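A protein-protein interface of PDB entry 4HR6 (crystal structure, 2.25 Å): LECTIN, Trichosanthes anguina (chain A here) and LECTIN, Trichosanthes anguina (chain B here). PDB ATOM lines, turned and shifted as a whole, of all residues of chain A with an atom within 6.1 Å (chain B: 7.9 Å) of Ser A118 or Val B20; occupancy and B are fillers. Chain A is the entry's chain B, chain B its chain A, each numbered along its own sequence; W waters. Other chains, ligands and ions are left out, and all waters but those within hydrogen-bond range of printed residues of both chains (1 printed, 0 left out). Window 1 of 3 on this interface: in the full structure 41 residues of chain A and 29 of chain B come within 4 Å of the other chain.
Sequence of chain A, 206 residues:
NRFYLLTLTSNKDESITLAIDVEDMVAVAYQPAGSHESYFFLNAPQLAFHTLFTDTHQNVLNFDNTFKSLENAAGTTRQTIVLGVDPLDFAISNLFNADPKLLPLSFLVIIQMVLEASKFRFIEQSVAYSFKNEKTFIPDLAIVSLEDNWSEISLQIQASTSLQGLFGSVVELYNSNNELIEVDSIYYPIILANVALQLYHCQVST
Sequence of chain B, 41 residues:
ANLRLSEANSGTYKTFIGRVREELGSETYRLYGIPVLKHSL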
ATOM      1  N   TYR A   4     -23.478  15.658  -3.745  1.00  0.00           N
ATOM      2  CA  TYR A   4     -22.359  14.922  -4.311  1.00  0.00           C
ATOM      3  C   TYR A   4     -22.321  15.190  -5.818  1.00  0.00           C
ATOM      4  O   TYR A   4     -23.361  15.142  -6.486  1.00  0.00           O
ATOM      5  CB  TYR A   4     -22.572  13.450  -4.027  1.00  0.00           C
ATOM      6  CG  TYR A   4     -21.501  12.514  -4.501  1.00  0.00           C
ATOM      7  CD1 TYR A   4     -20.204  12.581  -4.003  1.00  0.00           C
ATOM      8  CD2 TYR A   4     -21.800  11.513  -5.418  1.00  0.00           C
ATOM      9  CE1 TYR A   4     -19.231  11.676  -4.428  1.00  0.00           C
ATOM     10  CE2 TYR A   4     -20.844  10.617  -5.840  1.00  0.00           C
ATOM     11  CZ  TYR A   4     -19.567  10.695  -5.348  1.00  0.00           C
ATOM     12  OH  TYR A   4     -18.645   9.775  -5.804  1.00  0.00           O
ATOM     13  N   LEU A   6     -20.648  14.573  -9.705  1.00  0.00           N
ATOM     14  CA  LEU A   6     -20.366  13.405 -10.450  1.00  0.00           C
ATOM     15  C   LEU A   6     -20.260  13.821 -11.901  1.00  0.00           C
ATOM     16  O   LEU A   6     -21.178  14.438 -12.435  1.00  0.00           O
ATOM     17  CB  LEU A   6     -21.550  12.508 -10.204  1.00  0.00           C
ATOM     18  CG  LEU A   6     -21.410  11.067 -10.516  1.00  0.00           C
ATOM     19  CD1 LEU A   6     -22.224  10.314  -9.471  1.00  0.00           C
ATOM     20  CD2 LEU A   6     -21.893  10.865 -11.932  1.00  0.00           C
ATOM     21  N   MET A  25     -30.825  10.482  -2.219  1.00  0.00           N
ATOM     22  CA  MET A  25     -30.164   9.918  -3.380  1.00  0.00           C
ATOM     23  C   MET A  25     -30.938  10.140  -4.684  1.00  0.00           C
ATOM     24  O   MET A  25     -31.248   9.198  -5.416  1.00  0.00           O
ATOM     25  CB  MET A  25     -29.825   8.433  -3.173  1.00  0.00           C
ATOM     26  CG  MET A  25     -28.539   8.055  -3.923  1.00  0.00           C
ATOM     27  SD  MET A  25     -28.134   6.315  -3.812  1.00  0.00           S
ATOM     28  CE  MET A  25     -26.972   6.188  -5.171  1.00  0.00           C
ATOM     29  N   GLN A 112     -30.917   5.646 -14.259  1.00  0.00           N
ATOM     30  CA  GLN A 112     -30.927   4.198 -14.093  1.00  0.00           C
ATOM     31  C   GLN A 112     -29.536   3.597 -14.149  1.00  0.00           C
ATOM     32  O   GLN A 112     -29.178   2.787 -13.306  1.00  0.00           O
ATOM     33  CB  GLN A 112     -31.838   3.554 -15.111  1.00  0.00           C
ATOM     34  CG  GLN A 112     -33.290   3.847 -14.829  1.00  0.00           C
ATOM     35  CD  GLN A 112     -34.195   3.110 -15.762  1.00  0.00           C
ATOM     36  OE1 GLN A 112     -34.415   3.529 -16.900  1.00  0.00           O
ATOM     37  NE2 GLN A 112     -34.730   2.004 -15.292  1.00  0.00           N
ATOM     38  N   MET A 113     -28.739   4.027 -15.118  1.00  0.00           N
ATOM     39  CA  MET A 113     -27.429   3.440 -15.342  1.00  0.00           C
ATOM     40  C   MET A 113     -26.389   3.887 -14.334  1.00  0.00           C
ATOM     41  O   MET A 113     -25.345   3.230 -14.206  1.00  0.00           O
ATOM     42  CB  MET A 113     -26.939   3.747 -16.739  1.00  0.00           C
ATOM     43  CG  MET A 113     -27.679   2.982 -17.813  1.00  0.00           C
ATOM     44  SD  MET A 113     -27.071   3.301 -19.483  1.00  0.00           S
ATOM     45  CE  MET A 113     -25.472   2.480 -19.429  1.00  0.00           C
ATOM     46  N   VAL A 114     -26.660   4.965 -13.592  1.00  0.00           N
ATOM     47  CA  VAL A 114     -25.706   5.443 -12.590  1.00  0.00           C
ATOM     48  C   VAL A 114     -26.251   5.303 -11.163  1.00  0.00           C
ATOM     49  O   VAL A 114     -25.643   4.637 -10.319  1.00  0.00           O
ATOM     50  CB  VAL A 114     -25.307   6.910 -12.862  1.00  0.00           C
ATOM     51  CG1 VAL A 114     -24.384   7.408 -11.772  1.00  0.00           C
ATOM     52  CG2 VAL A 114     -24.621   7.028 -14.217  1.00  0.00           C
ATOM     53  N   LEU A 115     -27.406   5.907 -10.883  1.00  0.00           N
ATOM     54  CA  LEU A 115     -27.883   5.933  -9.520  1.00  0.00           C
ATOM     55  C   LEU A 115     -28.534   4.611  -9.147  1.00  0.00           C
ATOM     56  O   LEU A 115     -28.273   4.081  -8.087  1.00  0.00           O
ATOM     57  CB  LEU A 115     -28.852   7.095  -9.283  1.00  0.00           C
ATOM     58  CG  LEU A 115     -28.321   8.511  -9.484  1.00  0.00           C
ATOM     59  CD1 LEU A 115     -29.409   9.533  -9.149  1.00  0.00           C
ATOM     60  CD2 LEU A 115     -27.105   8.737  -8.611  1.00  0.00           C
ATOM     61  N   GLU A 116     -29.394   4.082 -10.008  1.00  0.00           N
ATOM     62  CA  GLU A 116     -30.106   2.860  -9.671  1.00  0.00           C
ATOM     63  C   GLU A 116     -29.157   1.649  -9.657  1.00  0.00           C
ATOM     64  O   GLU A 116     -29.296   0.741  -8.832  1.00  0.00           O
ATOM     65  CB  GLU A 116     -31.287   2.665 -10.615  1.00  0.00           C
ATOM     66  CG  GLU A 116     -32.283   3.822 -10.634  1.00  0.00           C
ATOM     67  CD  GLU A 116     -32.873   4.098  -9.282  1.00  0.00           C
ATOM     68  OE1 GLU A 116     -33.606   3.232  -8.785  1.00  0.00           O
ATOM     69  OE2 GLU A 116     -32.584   5.166  -8.691  1.00  0.00           O
ATOM     70  N   ALA A 117     -28.169   1.659 -10.547  1.00  0.00           N
ATOM     71  CA  ALA A 117     -27.126   0.638 -10.523  1.00  0.00           C
ATOM     72  C   ALA A 117     -26.325   0.687  -9.236  1.00  0.00           C
ATOM     73  O   ALA A 117     -25.874  -0.359  -8.768  1.00  0.00           O
ATOM     74  CB  ALA A 117     -26.202   0.796 -11.700  1.00  0.00           C
ATOM     75  N   SER A 118     -26.114   1.890  -8.679  1.00  0.00           N
ATOM     76  CA  SER A 118     -25.375   2.001  -7.426  1.00  0.00           C
ATOM     77  C   SER A 118     -26.155   1.394  -6.260  1.00  0.00           C
ATOM     78  O   SER A 118     -25.571   0.936  -5.292  1.00  0.00           O
ATOM     79  CB  SER A 118     -25.038   3.459  -7.114  1.00  0.00           C
ATOM     80  OG  SER A 118     -24.162   4.003  -8.103  1.00  0.00           O
ATOM     81  N   LYS A 119     -27.481   1.420  -6.345  1.00  0.00           N
ATOM     82  CA  LYS A 119     -28.325   0.949  -5.254  1.00  0.00           C
ATOM     83  C   LYS A 119     -28.415  -0.579  -5.221  1.00  0.00           C
ATOM     84  O   LYS A 119     -28.570  -1.168  -4.140  1.00  0.00           O
ATOM     85  CB  LYS A 119     -29.731   1.514  -5.409  1.00  0.00           C
ATOM     86  CG  LYS A 119     -29.857   3.020  -5.257  1.00  0.00           C
ATOM     87  CD  LYS A 119     -31.272   3.456  -5.620  1.00  0.00           C
ATOM     88  CE  LYS A 119     -31.491   4.934  -5.416  1.00  0.00           C
ATOM     89  NZ  LYS A 119     -32.831   5.328  -5.916  1.00  0.00           N
ATOM     90  N   PHE A 120     -28.370  -1.200  -6.406  1.00  0.00           N
ATOM     91  CA  PHE A 120     -28.655  -2.621  -6.570  1.00  0.00           C
ATOM     92  C   PHE A 120     -27.593  -3.334  -7.432  1.00  0.00           C
ATOM     93  O   PHE A 120     -27.372  -2.951  -8.572  1.00  0.00           O
ATOM     94  CB  PHE A 120     -30.005  -2.826  -7.244  1.00  0.00           C
ATOM     95  CG  PHE A 120     -31.173  -2.327  -6.447  1.00  0.00           C
ATOM     96  CD1 PHE A 120     -31.699  -3.083  -5.413  1.00  0.00           C
ATOM     97  CD2 PHE A 120     -31.748  -1.089  -6.732  1.00  0.00           C
ATOM     98  CE1 PHE A 120     -32.782  -2.628  -4.680  1.00  0.00           C
ATOM     99  CE2 PHE A 120     -32.827  -0.624  -6.002  1.00  0.00           C
ATOM    100  CZ  PHE A 120     -33.348  -1.399  -4.974  1.00  0.00           C
ATOM    101  N   ARG A 121     -26.986  -4.386  -6.880  1.00  0.00           N
ATOM    102  CA  ARG A 121     -26.060  -5.261  -7.606  1.00  0.00           C
ATOM    103  C   ARG A 121     -26.692  -5.872  -8.856  1.00  0.00           C
ATOM    104  O   ARG A 121     -26.061  -5.926  -9.900  1.00  0.00           O
ATOM    105  CB  ARG A 121     -25.522  -6.357  -6.680  1.00  0.00           C
ATOM    106  CG  ARG A 121     -24.588  -5.839  -5.583  1.00  0.00           C
ATOM    107  CD  ARG A 121     -23.571  -6.915  -5.158  1.00  0.00           C
ATOM    108  NE  ARG A 121     -22.581  -6.383  -4.227  1.00  0.00           N
ATOM    109  CZ  ARG A 121     -22.731  -6.294  -2.898  1.00  0.00           C
ATOM    110  NH1 ARG A 121     -23.839  -6.725  -2.293  1.00  0.00           N
ATOM    111  NH2 ARG A 121     -21.752  -5.775  -2.157  1.00  0.00           N
ATOM    112  N   ILE A 123     -28.852  -4.562 -10.846  1.00  0.00           N
ATOM    113  CA  ILE A 123     -28.918  -3.558 -11.901  1.00  0.00           C
ATOM    114  C   ILE A 123     -27.515  -3.240 -12.389  1.00  0.00           C
ATOM    115  O   ILE A 123     -27.278  -3.138 -13.568  1.00  0.00           O
ATOM    116  CB  ILE A 123     -29.670  -2.274 -11.451  1.00  0.00           C
ATOM    117  CG1 ILE A 123     -31.122  -2.615 -11.152  1.00  0.00           C
ATOM    118  CG2 ILE A 123     -29.619  -1.203 -12.540  1.00  0.00           C
ATOM    119  CD1 ILE A 123     -31.894  -1.471 -10.523  1.00  0.00           C
ATOM    120  N   GLU A 124     -26.589  -3.086 -11.480  1.00  0.00           N
ATOM    121  CA  GLU A 124     -25.192  -2.960 -11.856  1.00  0.00           C
ATOM    122  C   GLU A 124     -24.764  -4.066 -12.844  1.00  0.00           C
ATOM    123  O   GLU A 124     -24.148  -3.783 -13.879  1.00  0.00           O
ATOM    124  CB  GLU A 124     -24.327  -3.026 -10.616  1.00  0.00           C
ATOM    125  CG  GLU A 124     -22.841  -2.827 -10.880  1.00  0.00           C
ATOM    126  CD  GLU A 124     -21.985  -3.258  -9.708  1.00  0.00           C
ATOM    127  OE1 GLU A 124     -20.753  -3.027  -9.751  1.00  0.00           O
ATOM    128  OE2 GLU A 124     -22.545  -3.801  -8.735  1.00  0.00           O
ATOM    129  N   ALA A 196     -27.227  -2.449  -2.137  1.00  0.00           N
ATOM    130  CA  ALA A 196     -25.868  -2.025  -1.793  1.00  0.00           C
ATOM    131  C   ALA A 196     -25.858  -0.744  -1.017  1.00  0.00           C
ATOM    132  O   ALA A 196     -24.877  -0.459  -0.353  1.00  0.00           O
ATOM    133  CB  ALA A 196     -24.994  -1.893  -3.047  1.00  0.00           C
ATOM    134  N   LEU A 197     -26.941   0.038  -1.109  1.00  0.00           N
ATOM    135  CA  LEU A 197     -27.079   1.282  -0.363  1.00  0.00           C
ATOM    136  C   LEU A 197     -28.506   1.383   0.130  1.00  0.00           C
ATOM    137  O   LEU A 197     -29.424   1.030  -0.596  1.00  0.00           O
ATOM    138  CB  LEU A 197     -26.799   2.482  -1.258  1.00  0.00           C
ATOM    139  CG  LEU A 197     -25.364   2.741  -1.698  1.00  0.00           C
ATOM    140  CD1 LEU A 197     -25.338   3.909  -2.674  1.00  0.00           C
ATOM    141  CD2 LEU A 197     -24.426   2.998  -0.537  1.00  0.00           C
ATOM    142  N   ALA B   1     -15.634  11.522  -8.672  1.00  0.00           N
ATOM    143  CA  ALA B   1     -16.150  10.342  -9.434  1.00  0.00           C
ATOM    144  C   ALA B   1     -16.506  10.746 -10.869  1.00  0.00           C
ATOM    145  O   ALA B   1     -17.307  11.662 -11.098  1.00  0.00           O
ATOM    146  CB  ALA B   1     -17.350   9.738  -8.733  1.00  0.00           C
ATOM    147  N   ASN B   2     -15.886  10.060 -11.822  1.00  0.00           N
ATOM    148  CA  ASN B   2     -15.940  10.429 -13.233  1.00  0.00           C
ATOM    149  C   ASN B   2     -16.066   9.162 -14.068  1.00  0.00           C
ATOM    150  O   ASN B   2     -15.466   8.145 -13.740  1.00  0.00           O
ATOM    151  CB  ASN B   2     -14.674  11.213 -13.618  1.00  0.00           C
ATOM    152  CG  ASN B   2     -14.629  11.601 -15.105  1.00  0.00           C
ATOM    153  OD1 ASN B   2     -15.646  11.960 -15.721  1.00  0.00           O
ATOM    154  ND2 ASN B   2     -13.434  11.538 -15.686  1.00  0.00           N
ATOM    155  N   TYR B  13     -16.631   0.511 -15.672  1.00  0.00           N
ATOM    156  CA  TYR B  13     -17.983   0.802 -15.209  1.00  0.00           C
ATOM    157  C   TYR B  13     -18.180   0.357 -13.752  1.00  0.00           C
ATOM    158  O   TYR B  13     -18.554   1.162 -12.909  1.00  0.00           O
ATOM    159  CB  TYR B  13     -19.023   0.158 -16.123  1.00  0.00           C
ATOM    160  CG  TYR B  13     -20.431   0.303 -15.586  1.00  0.00           C
ATOM    161  CD1 TYR B  13     -21.070   1.545 -15.587  1.00  0.00           C
ATOM    162  CD2 TYR B  13     -21.101  -0.779 -15.035  1.00  0.00           C
ATOM    163  CE1 TYR B  13     -22.339   1.702 -15.079  1.00  0.00           C
ATOM    164  CE2 TYR B  13     -22.385  -0.638 -14.527  1.00  0.00           C
ATOM    165  CZ  TYR B  13     -22.993   0.610 -14.541  1.00  0.00           C
ATOM    166  OH  TYR B  13     -24.257   0.757 -14.032  1.00  0.00           O
ATOM    167  N   LYS B  14     -17.853  -0.897 -13.443  1.00  0.00           N
ATOM    168  CA  LYS B  14     -17.982  -1.436 -12.072  1.00  0.00           C
ATOM    169  C   LYS B  14     -17.116  -0.725 -11.049  1.00  0.00           C
ATOM    170  O   LYS B  14     -17.526  -0.547  -9.910  1.00  0.00           O
ATOM    171  CB  LYS B  14     -17.632  -2.909 -12.022  1.00  0.00           C
ATOM    172  CG  LYS B  14     -18.638  -3.798 -12.702  1.00  0.00           C
ATOM    173  CD  LYS B  14     -18.222  -5.249 -12.529  1.00  0.00           C
ATOM    174  CE  LYS B  14     -18.982  -6.170 -13.462  1.00  0.00           C
ATOM    175  NZ  LYS B  14     -18.339  -7.520 -13.535  1.00  0.00           N
ATOM    176  N   THR B  15     -15.911  -0.337 -11.453  1.00  0.00           N
ATOM    177  CA  THR B  15     -15.030   0.467 -10.601  1.00  0.00           C
ATOM    178  C   THR B  15     -15.641   1.827 -10.252  1.00  0.00           C
ATOM    179  O   THR B  15     -15.556   2.292  -9.122  1.00  0.00           O
ATOM    180  CB  THR B  15     -13.680   0.683 -11.314  1.00  0.00           C
ATOM    181  OG1 THR B  15     -13.069  -0.592 -11.536  1.00  0.00           O
ATOM    182  CG2 THR B  15     -12.753   1.534 -10.510  1.00  0.00           C
ATOM    183  N   PHE B  16     -16.207   2.480 -11.256  1.00  0.00           N
ATOM    184  CA  PHE B  16     -16.942   3.727 -11.081  1.00  0.00           C
ATOM    185  C   PHE B  16     -18.130   3.570 -10.103  1.00  0.00           C
ATOM    186  O   PHE B  16     -18.240   4.325  -9.159  1.00  0.00           O
ATOM    187  CB  PHE B  16     -17.423   4.219 -12.456  1.00  0.00           C
ATOM    188  CG  PHE B  16     -18.427   5.319 -12.397  1.00  0.00           C
ATOM    189  CD1 PHE B  16     -18.038   6.614 -12.088  1.00  0.00           C
ATOM    190  CD2 PHE B  16     -19.753   5.069 -12.680  1.00  0.00           C
ATOM    191  CE1 PHE B  16     -18.959   7.634 -12.058  1.00  0.00           C
ATOM    192  CE2 PHE B  16     -20.688   6.085 -12.653  1.00  0.00           C
ATOM    193  CZ  PHE B  16     -20.289   7.371 -12.335  1.00  0.00           C
ATOM    194  N   ILE B  17     -18.989   2.580 -10.331  1.00  0.00           N
ATOM    195  CA  ILE B  17     -20.111   2.314  -9.425  1.00  0.00           C
ATOM    196  C   ILE B  17     -19.578   2.004  -8.031  1.00  0.00           C
ATOM    197  O   ILE B  17     -20.134   2.452  -7.016  1.00  0.00           O
ATOM    198  CB  ILE B  17     -20.995   1.164  -9.920  1.00  0.00           C
ATOM    199  CG1 ILE B  17     -21.693   1.536 -11.234  1.00  0.00           C
ATOM    200  CG2 ILE B  17     -22.017   0.758  -8.848  1.00  0.00           C
ATOM    201  CD1 ILE B  17     -22.660   2.708 -11.161  1.00  0.00           C
ATOM    202  N   GLY B  18     -18.469   1.272  -7.988  1.00  0.00           N
ATOM    203  CA  GLY B  18     -17.817   0.964  -6.719  1.00  0.00           C
ATOM    204  C   GLY B  18     -17.403   2.198  -5.960  1.00  0.00           C
ATOM    205  O   GLY B  18     -17.593   2.270  -4.743  1.00  0.00           O
ATOM    206  N   ARG B  19     -16.849   3.176  -6.674  1.00  0.00           N
ATOM    207  CA  ARG B  19     -16.444   4.429  -6.044  1.00  0.00           C
ATOM    208  C   ARG B  19     -17.659   5.286  -5.583  1.00  0.00           C
ATOM    209  O   ARG B  19     -17.610   5.933  -4.535  1.00  0.00           O
ATOM    210  CB  ARG B  19     -15.491   5.231  -6.960  1.00  0.00           C
ATOM    211  CG  ARG B  19     -15.132   6.617  -6.408  1.00  0.00           C
ATOM    212  CD  ARG B  19     -13.637   6.922  -6.371  1.00  0.00           C
ATOM    213  NE  ARG B  19     -13.227   7.870  -7.415  1.00  0.00           N
ATOM    214  CZ  ARG B  19     -13.092   9.193  -7.263  1.00  0.00           C
ATOM    215  NH1 ARG B  19     -13.329   9.793  -6.097  1.00  0.00           N
ATOM    216  NH2 ARG B  19     -12.711   9.931  -8.305  1.00  0.00           N
ATOM    217  N   VAL B  20     -18.739   5.298  -6.356  1.00  0.00           N
ATOM    218  CA  VAL B  20     -19.933   6.023  -5.945  1.00  0.00           C
ATOM    219  C   VAL B  20     -20.438   5.446  -4.612  1.00  0.00           C
ATOM    220  O   VAL B  20     -20.656   6.199  -3.672  1.00  0.00           O
ATOM    221  CB  VAL B  20     -21.019   5.993  -7.021  1.00  0.00           C
ATOM    222  CG1 VAL B  20     -22.357   6.494  -6.483  1.00  0.00           C
ATOM    223  CG2 VAL B  20     -20.587   6.824  -8.208  1.00  0.00           C
ATOM    224  N   ARG B  21     -20.557   4.122  -4.535  1.00  0.00           N
ATOM    225  CA  ARG B  21     -20.991   3.427  -3.306  1.00  0.00           C
ATOM    226  C   ARG B  21     -20.118   3.724  -2.096  1.00  0.00           C
ATOM    227  O   ARG B  21     -20.630   3.929  -1.000  1.00  0.00           O
ATOM    228  CB  ARG B  21     -21.038   1.907  -3.519  1.00  0.00           C
ATOM    229  CG  ARG B  21     -22.139   1.475  -4.457  1.00  0.00           C
ATOM    230  CD  ARG B  21     -22.096  -0.017  -4.667  1.00  0.00           C
ATOM    231  NE  ARG B  21     -23.174  -0.453  -5.537  1.00  0.00           N
ATOM    232  CZ  ARG B  21     -23.127  -1.533  -6.303  1.00  0.00           C
ATOM    233  NH1 ARG B  21     -22.025  -2.284  -6.367  1.00  0.00           N
ATOM    234  NH2 ARG B  21     -24.161  -1.844  -7.053  1.00  0.00           N
ATOM    235  N   GLU B  22     -18.806   3.752  -2.293  1.00  0.00           N
ATOM    236  CA  GLU B  22     -17.875   3.993  -1.194  1.00  0.00           C
ATOM    237  C   GLU B  22     -17.962   5.419  -0.671  1.00  0.00           C
ATOM    238  O   GLU B  22     -17.820   5.664   0.537  1.00  0.00           O
ATOM    239  CB  GLU B  22     -16.449   3.697  -1.646  1.00  0.00           C
ATOM    240  CG  GLU B  22     -15.410   3.767  -0.542  1.00  0.00           C
ATOM    241  CD  GLU B  22     -13.998   3.482  -1.045  1.00  0.00           C
ATOM    242  OE1 GLU B  22     -13.837   2.731  -2.041  1.00  0.00           O
ATOM    243  OE2 GLU B  22     -13.044   4.019  -0.436  1.00  0.00           O
ATOM    244  N   GLU B  23     -18.165   6.367  -1.571  1.00  0.00           N
ATOM    245  CA  GLU B  23     -18.254   7.761  -1.164  1.00  0.00           C
ATOM    246  C   GLU B  23     -19.624   8.131  -0.567  1.00  0.00           C
ATOM    247  O   GLU B  23     -19.696   9.038   0.242  1.00  0.00           O
ATOM    248  CB  GLU B  23     -17.898   8.696  -2.322  1.00  0.00           C
ATOM    249  CG  GLU B  23     -16.396   8.766  -2.588  1.00  0.00           C
ATOM    250  CD  GLU B  23     -16.026   9.824  -3.613  1.00  0.00           C
ATOM    251  OE1 GLU B  23     -16.311   9.626  -4.813  1.00  0.00           O
ATOM    252  OE2 GLU B  23     -15.455  10.863  -3.216  1.00  0.00           O
ATOM    253  N   LEU B  24     -20.698   7.445  -0.968  1.00  0.00           N
ATOM    254  CA  LEU B  24     -22.049   7.753  -0.460  1.00  0.00           C
ATOM    255  C   LEU B  24     -22.476   6.932   0.776  1.00  0.00           C
ATOM    256  O   LEU B  24     -23.288   7.403   1.585  1.00  0.00           O
ATOM    257  CB  LEU B  24     -23.083   7.565  -1.563  1.00  0.00           C
ATOM    258  CG  LEU B  24     -23.018   8.568  -2.716  1.00  0.00           C
ATOM    259  CD1 LEU B  24     -24.119   8.252  -3.710  1.00  0.00           C
ATOM    260  CD2 LEU B  24     -23.142   9.996  -2.221  1.00  0.00           C
ATOM    261  N   GLY B  25     -21.949   5.712   0.888  1.00  0.00           N
ATOM    262  CA  GLY B  25     -22.291   4.796   1.951  1.00  0.00           C
ATOM    263  C   GLY B  25     -21.502   5.080   3.218  1.00  0.00           C
ATOM    264  O   GLY B  25     -20.295   5.317   3.169  1.00  0.00           O
ATOM    265  N   LEU B  37     -26.937   5.464   3.769  1.00  0.00           N
ATOM    266  CA  LEU B  37     -26.340   6.644   3.171  1.00  0.00           C
ATOM    267  C   LEU B  37     -25.861   7.604   4.242  1.00  0.00           C
ATOM    268  O   LEU B  37     -26.495   7.750   5.301  1.00  0.00           O
ATOM    269  CB  LEU B  37     -27.321   7.375   2.259  1.00  0.00           C
ATOM    270  CG  LEU B  37     -27.702   6.632   0.984  1.00  0.00           C
ATOM    271  CD1 LEU B  37     -28.977   7.188   0.380  1.00  0.00           C
ATOM    272  CD2 LEU B  37     -26.557   6.705   0.002  1.00  0.00           C
ATOM    273  N   LYS B  38     -24.741   8.258   3.963  1.00  0.00           N
ATOM    274  CA  LYS B  38     -24.188   9.270   4.863  1.00  0.00           C
ATOM    275  C   LYS B  38     -25.105  10.465   4.947  1.00  0.00           C
ATOM    276  O   LYS B  38     -25.821  10.764   4.003  1.00  0.00           O
ATOM    277  CB  LYS B  38     -22.845   9.770   4.337  1.00  0.00           C
ATOM    278  CG  LYS B  38     -21.720   8.770   4.390  1.00  0.00           C
ATOM    279  CD  LYS B  38     -20.426   9.408   3.890  1.00  0.00           C
ATOM    280  CE  LYS B  38     -19.338   8.361   3.751  1.00  0.00           C
ATOM    281  NZ  LYS B  38     -18.215   8.894   2.955  1.00  0.00           N
ATOM    282  N   LEU B  41     -21.186  14.995   3.459  1.00  0.00           N
ATOM    283  CA  LEU B  41     -19.860  14.734   2.922  1.00  0.00           C
ATOM    284  C   LEU B  41     -18.869  15.738   3.509  1.00  0.00           C
ATOM    285  O   LEU B  41     -18.372  15.559   4.626  1.00  0.00           O
ATOM    286  CB  LEU B  41     -19.897  14.861   1.400  1.00  0.00           C
ATOM    287  CG  LEU B  41     -20.935  13.977   0.702  1.00  0.00           C
ATOM    288  CD1 LEU B  41     -21.071  14.364  -0.761  1.00  0.00           C
ATOM    289  CD2 LEU B  41     -20.575  12.508   0.837  1.00  0.00           C
HETATM  290  O   HOH W   1     -18.850  -2.352  -8.350  1.00  0.00           O
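The side-chain carboxylate of Glu A124 is in salt-bridge range of the guanidinium group of Arg B21 (2.9 Å). The guanidinium group of Arg B21 sits at hydrogen-bond distance from the backbone carbonyl oxygen of Ala A117, at 2.8 Å. The guanidinium group (NE) of Arg B21 sits at hydrogen-bond distance from the backbone carbonyl oxygen (O) of Ser A118 (2.8 Å). O of Met A113 sits at hydrogen-bond distance from OH of Tyr B13 (2.7 Å). The side-chain carboxylate of Glu B23 lies within hydrogen-bond range of the side-chain hydroxyl of Tyr A4.
The backbone carbonyl oxygen of Val A114 lies within hydrogen-bond range of the side-chain hydroxyl of Ser A118 (2.7 Å). The backbone carbonyl oxygen of Lys A119 sits at hydrogen-bond distance from the backbone NH of Ala A196 (2.7 Å). O of Leu B24 is in hydrogen-bond range of N of Lys B38 (2.9 Å). NH1 of Arg B19 is in salt-bridge range of OE1 of Glu B23 (3.3 Å). The backbone carbonyl oxygen of Gln A112 lies within hydrogen-bond range of the backbone NH of Ala A117 (3.1 Å). NZ of Lys B38 is in hydrogen-bond range of O of Glu B23 (3.1 Å).
Tyr A4 touches Ala B1 (OH to CB, 3.2 Å). Leu B24 touches Tyr A4. Met A25 touches Leu B24. Ala A117 touches Tyr B13. Ser A118 touches Ile B17. Ser A118 touches Val B20. O of Phe A120 touches NH2 of Arg B21, 3.7 Å away. Arg B21 touches Arg A121 (NH2 to N, 3.8 Å). CE2 of Tyr B13 touches O of Glu A124, at 3.7 Å. OE1 of Glu A124 touches CG of Lys B14, at 3.7 Å.
Of the printed residues of chain B, Ser A118 touches Ile B17 (3.6 Å), Val B20 (3.5 Å) and Arg B21 (2.8 Å). Val B20 touches just these residues of chain A: Tyr A4 and Ser A118. Printed residues of chain B within 4 Å of Ala A117: Tyr B13 (3.0 Å) and Arg B21 (2.8 Å). Of the printed residues of chain A, Leu B24 touches Tyr A4 (3.8 Å) and Met A25 (3.8 Å). Of the printed residues of chain A, Lys B14 touches Glu A124 (3.7 Å). Of the printed residues of chain A, Tyr B13 touches Met A113 (2.7 Å), Ala A117 (3.0 Å) and Glu A124 (3.7 Å). Printed residues of chain A within 4 Å of Glu B23: Tyr A4 (2.5 Å).
Of the 18 printed residues of chain B, 12 touch a printed residue of chain A. Hydrophobic or aromatic side chains of chain B that line the printed part of chain A: Ala B1, Tyr B13, Phe B16, Ile B17, Val B20, Leu B24, Leu B37 and Leu B41. Among the printed residues, 24 pairs touch across the chains. Among the printed residues, Asp or Glu carboxylates within 4 Å of a Lys or Arg side-chain nitrogen of the other chain: Glu A124 with Arg B21.
Water W1 bridges the side-chain carboxylate of Glu A124 (2.5 Å) and the backbone carbonyl oxygen of Lys B14 (2.7 Å).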
